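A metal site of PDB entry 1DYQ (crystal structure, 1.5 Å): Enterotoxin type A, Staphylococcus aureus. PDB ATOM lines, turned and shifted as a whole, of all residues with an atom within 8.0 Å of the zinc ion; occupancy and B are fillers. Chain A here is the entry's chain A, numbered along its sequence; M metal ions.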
ATOM      1  N   PRO A 127      -5.819 -24.899  -6.512  1.00  0.00           N
ATOM      2  CA  PRO A 127      -7.140 -25.452  -6.182  1.00  0.00           C
ATOM      3  C   PRO A 127      -7.407 -25.328  -4.690  1.00  0.00           C
ATOM      4  O   PRO A 127      -6.497 -25.499  -3.864  1.00  0.00           O
ATOM      5  CB  PRO A 127      -7.040 -26.892  -6.634  1.00  0.00           C
ATOM      6  CG  PRO A 127      -5.914 -26.960  -7.579  1.00  0.00           C
ATOM      7  CD  PRO A 127      -4.916 -25.892  -7.093  1.00  0.00           C
ATOM      8  N   ASN A 129     -10.032 -26.753  -1.666  1.00  0.00           N
ATOM      9  CA  ASN A 129     -11.141 -27.584  -1.148  1.00  0.00           C
ATOM     10  C   ASN A 129     -11.715 -26.810   0.057  1.00  0.00           C
ATOM     11  O   ASN A 129     -10.978 -26.595   1.022  1.00  0.00           O
ATOM     12  CB  ASN A 129     -10.636 -28.927  -0.675  1.00  0.00           C
ATOM     13  CG  ASN A 129      -9.930 -29.732  -1.760  1.00  0.00           C
ATOM     14  OD1 ASN A 129      -8.812 -30.186  -1.568  1.00  0.00           O
ATOM     15  ND2 ASN A 129     -10.584 -29.848  -2.904  1.00  0.00           N
ATOM     16  N   TRP A 131     -14.836 -26.640   2.904  1.00  0.00           N
ATOM     17  CA  TRP A 131     -16.010 -27.240   3.568  1.00  0.00           C
ATOM     18  C   TRP A 131     -16.613 -26.208   4.527  1.00  0.00           C
ATOM     19  O   TRP A 131     -15.864 -25.524   5.243  1.00  0.00           O
ATOM     20  CB  TRP A 131     -15.615 -28.490   4.324  1.00  0.00           C
ATOM     21  CG  TRP A 131     -15.215 -29.653   3.457  1.00  0.00           C
ATOM     22  CD1 TRP A 131     -16.040 -30.620   2.978  1.00  0.00           C
ATOM     23  CD2 TRP A 131     -13.891 -29.993   3.034  1.00  0.00           C
ATOM     24  NE1 TRP A 131     -15.325 -31.541   2.257  1.00  0.00           N
ATOM     25  CE2 TRP A 131     -13.991 -31.197   2.292  1.00  0.00           C
ATOM     26  CE3 TRP A 131     -12.621 -29.436   3.212  1.00  0.00           C
ATOM     27  CZ2 TRP A 131     -12.892 -31.805   1.708  1.00  0.00           C
ATOM     28  CZ3 TRP A 131     -11.537 -30.041   2.634  1.00  0.00           C
ATOM     29  CH2 TRP A 131     -11.665 -31.233   1.881  1.00  0.00           C
ATOM     30  N   VAL A 186      -5.266 -24.716   5.476  1.00  0.00           N
ATOM     31  CA  VAL A 186      -4.110 -25.592   5.316  1.00  0.00           C
ATOM     32  C   VAL A 186      -3.548 -25.443   3.906  1.00  0.00           C
ATOM     33  O   VAL A 186      -4.235 -25.501   2.896  1.00  0.00           O
ATOM     34  CB  VAL A 186      -4.524 -27.071   5.529  1.00  0.00           C
ATOM     35  CG1 VAL A 186      -3.340 -28.001   5.390  1.00  0.00           C
ATOM     36  CG2 VAL A 186      -5.183 -27.266   6.887  1.00  0.00           C
ATOM     37  N   PHE A 187      -2.225 -25.237   3.881  1.00  0.00           N
ATOM     38  CA  PHE A 187      -1.480 -25.105   2.628  1.00  0.00           C
ATOM     39  C   PHE A 187      -0.780 -26.446   2.370  1.00  0.00           C
ATOM     40  O   PHE A 187       0.204 -26.812   2.944  1.00  0.00           O
ATOM     41  CB  PHE A 187      -0.457 -23.939   2.765  1.00  0.00           C
ATOM     42  CG  PHE A 187      -1.159 -22.638   3.088  1.00  0.00           C
ATOM     43  CD1 PHE A 187      -1.691 -21.848   2.134  1.00  0.00           C
ATOM     44  CD2 PHE A 187      -1.279 -22.275   4.447  1.00  0.00           C
ATOM     45  CE1 PHE A 187      -2.389 -20.677   2.431  1.00  0.00           C
ATOM     46  CE2 PHE A 187      -2.002 -21.103   4.761  1.00  0.00           C
ATOM     47  CZ  PHE A 187      -2.536 -20.333   3.783  1.00  0.00           C
ATOM     48  N   HIS A 188      -1.538 -27.259   1.580  1.00  0.00           N
ATOM     49  CA  HIS A 188      -1.212 -28.678   1.479  1.00  0.00           C
ATOM     50  C   HIS A 188      -0.262 -28.986   0.334  1.00  0.00           C
ATOM     51  O   HIS A 188      -0.651 -29.087  -0.811  1.00  0.00           O
ATOM     52  CB  HIS A 188      -2.500 -29.508   1.318  1.00  0.00           C
ATOM     53  CG  HIS A 188      -2.270 -30.964   1.669  1.00  0.00           C
ATOM     54  ND1 HIS A 188      -3.378 -31.762   1.832  1.00  0.00           N
ATOM     55  CD2 HIS A 188      -1.238 -31.732   1.952  1.00  0.00           C
ATOM     56  CE1 HIS A 188      -3.038 -32.992   2.139  1.00  0.00           C
ATOM     57  NE2 HIS A 188      -1.708 -33.001   2.222  1.00  0.00           N
ATOM     58  N   THR A 189       1.014 -29.105   0.675  1.00  0.00           N
ATOM     59  CA  THR A 189       2.067 -29.339  -0.294  1.00  0.00           C
ATOM     60  C   THR A 189       2.282 -30.821  -0.566  1.00  0.00           C
ATOM     61  O   THR A 189       1.910 -31.650   0.264  1.00  0.00           O
ATOM     62  CB  THR A 189       3.407 -28.750   0.266  1.00  0.00           C
ATOM     63  OG1 THR A 189       3.448 -29.064   1.683  1.00  0.00           O
ATOM     64  CG2 THR A 189       3.391 -27.239   0.123  1.00  0.00           C
ATOM     65  N   SER A 194       2.429 -29.767   6.112  1.00  0.00           N
ATOM     66  CA  SER A 194       1.665 -28.617   5.660  1.00  0.00           C
ATOM     67  C   SER A 194       1.616 -27.522   6.720  1.00  0.00           C
ATOM     68  O   SER A 194       1.363 -27.782   7.905  1.00  0.00           O
ATOM     69  CB  SER A 194       0.241 -29.063   5.296  1.00  0.00           C
ATOM     70  OG  SER A 194       0.318 -30.034   4.249  1.00  0.00           O
ATOM     71  N   MET A 225       0.401 -28.177  -5.539  1.00  0.00           N
ATOM     72  CA  MET A 225      -0.164 -27.979  -4.175  1.00  0.00           C
ATOM     73  C   MET A 225      -1.602 -27.568  -4.249  1.00  0.00           C
ATOM     74  O   MET A 225      -2.167 -27.230  -5.293  1.00  0.00           O
ATOM     75  CB  MET A 225       0.694 -26.873  -3.554  1.00  0.00           C
ATOM     76  CG  MET A 225       0.293 -26.443  -2.170  1.00  0.00           C
ATOM     77  SD  MET A 225      -0.514 -24.787  -2.098  1.00  0.00           S
ATOM     78  CE  MET A 225       0.644 -23.914  -3.125  1.00  0.00           C
ATOM     79  N   HIS A 226      -2.284 -27.659  -3.083  1.00  0.00           N
ATOM     80  CA  HIS A 226      -3.646 -27.077  -3.056  1.00  0.00           C
ATOM     81  C   HIS A 226      -3.908 -26.586  -1.619  1.00  0.00           C
ATOM     82  O   HIS A 226      -3.075 -26.786  -0.759  1.00  0.00           O
ATOM     83  CB  HIS A 226      -4.690 -28.097  -3.495  1.00  0.00           C
ATOM     84  CG  HIS A 226      -4.792 -29.243  -2.558  1.00  0.00           C
ATOM     85  ND1 HIS A 226      -4.075 -30.407  -2.708  1.00  0.00           N
ATOM     86  CD2 HIS A 226      -5.492 -29.375  -1.398  1.00  0.00           C
ATOM     87  CE1 HIS A 226      -4.313 -31.224  -1.699  1.00  0.00           C
ATOM     88  NE2 HIS A 226      -5.157 -30.613  -0.930  1.00  0.00           N
ATOM     89  N   ILE A 227      -5.026 -25.925  -1.447  1.00  0.00           N
ATOM     90  CA  ILE A 227      -5.370 -25.342  -0.150  1.00  0.00           C
ATOM     91  C   ILE A 227      -6.692 -25.997   0.343  1.00  0.00           C
ATOM     92  O   ILE A 227      -7.607 -26.107  -0.448  1.00  0.00           O
ATOM     93  CB  ILE A 227      -5.587 -23.823  -0.337  1.00  0.00           C
ATOM     94  CG1 ILE A 227      -4.192 -23.168  -0.499  1.00  0.00           C
ATOM     95  CG2 ILE A 227      -6.297 -23.231   0.874  1.00  0.00           C
ATOM     96  CD1 ILE A 227      -4.276 -21.726  -0.984  1.00  0.00           C
ATOM     97  N   ASP A 228      -6.719 -26.245   1.634  1.00  0.00           N
ATOM     98  CA  ASP A 228      -7.929 -26.755   2.270  1.00  0.00           C
ATOM     99  C   ASP A 228      -8.430 -25.733   3.312  1.00  0.00           C
ATOM    100  O   ASP A 228      -7.627 -25.251   4.102  1.00  0.00           O
ATOM    101  CB  ASP A 228      -7.695 -28.075   3.018  1.00  0.00           C
ATOM    102  CG  ASP A 228      -7.127 -29.130   2.108  1.00  0.00           C
ATOM    103  OD1 ASP A 228      -7.677 -29.400   1.026  1.00  0.00           O
ATOM    104  OD2 ASP A 228      -6.018 -29.546   2.506  1.00  0.00           O
ATOM    105  N   ILE A 229      -9.709 -25.463   3.235  1.00  0.00           N
ATOM    106  CA  ILE A 229     -10.332 -24.521   4.168  1.00  0.00           C
ATOM    107  C   ILE A 229     -11.521 -25.203   4.858  1.00  0.00           C
ATOM    108  O   ILE A 229     -12.373 -25.751   4.123  1.00  0.00           O
ATOM    109  CB  ILE A 229     -10.771 -23.252   3.416  1.00  0.00           C
ATOM    110  CG1 ILE A 229      -9.501 -22.504   2.901  1.00  0.00           C
ATOM    111  CG2 ILE A 229     -11.519 -22.318   4.373  1.00  0.00           C
ATOM    112  CD1 ILE A 229      -9.826 -21.334   2.016  1.00  0.00           C
ATOM    113  N   TYR A 230     -11.524 -25.208   6.148  1.00  0.00           N
ATOM    114  CA  TYR A 230     -12.624 -25.772   6.956  1.00  0.00           C
ATOM    115  C   TYR A 230     -13.258 -24.643   7.772  1.00  0.00           C
ATOM    116  O   TYR A 230     -12.567 -24.046   8.597  1.00  0.00           O
ATOM    117  CB  TYR A 230     -12.058 -26.823   7.908  1.00  0.00           C
ATOM    118  CG  TYR A 230     -11.181 -27.870   7.246  1.00  0.00           C
ATOM    119  CD1 TYR A 230      -9.810 -27.689   7.108  1.00  0.00           C
ATOM    120  CD2 TYR A 230     -11.744 -29.039   6.725  1.00  0.00           C
ATOM    121  CE1 TYR A 230      -9.023 -28.618   6.473  1.00  0.00           C
ATOM    122  CE2 TYR A 230     -10.946 -29.988   6.114  1.00  0.00           C
ATOM    123  CZ  TYR A 230      -9.600 -29.776   5.990  1.00  0.00           C
ATOM    124  OH  TYR A 230      -8.785 -30.704   5.359  1.00  0.00           O
HETATM  125 ZN    ZN M   1      -5.474 -31.196   1.192  1.00  0.00          ZN
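Three residues have an atom within 4 Å of the zinc ion: His 188, His 226 and Asp 228. The nearest printed residue that does not touch the zinc ion is Asn 129 (4.4 Å).
The zinc ion is bound by the side-chain carboxylate (OD2) of Asp 228, a ring nitrogen (NE2) of His 226 and a ring nitrogen (ND1) of His 188. The zinc ion has three donor atoms within binding distance. Slightly farther from the zinc ion lies OD1 of Asp 228 (2.8 Å).
OD1 of Asp 228 sits close to OD1 of Asn 129, 2.9 Å away. The backbone NH (N) of Val 186 lies within hydrogen-bond range of the backbone carbonyl oxygen (O) of Asp 228 (2.8 Å).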
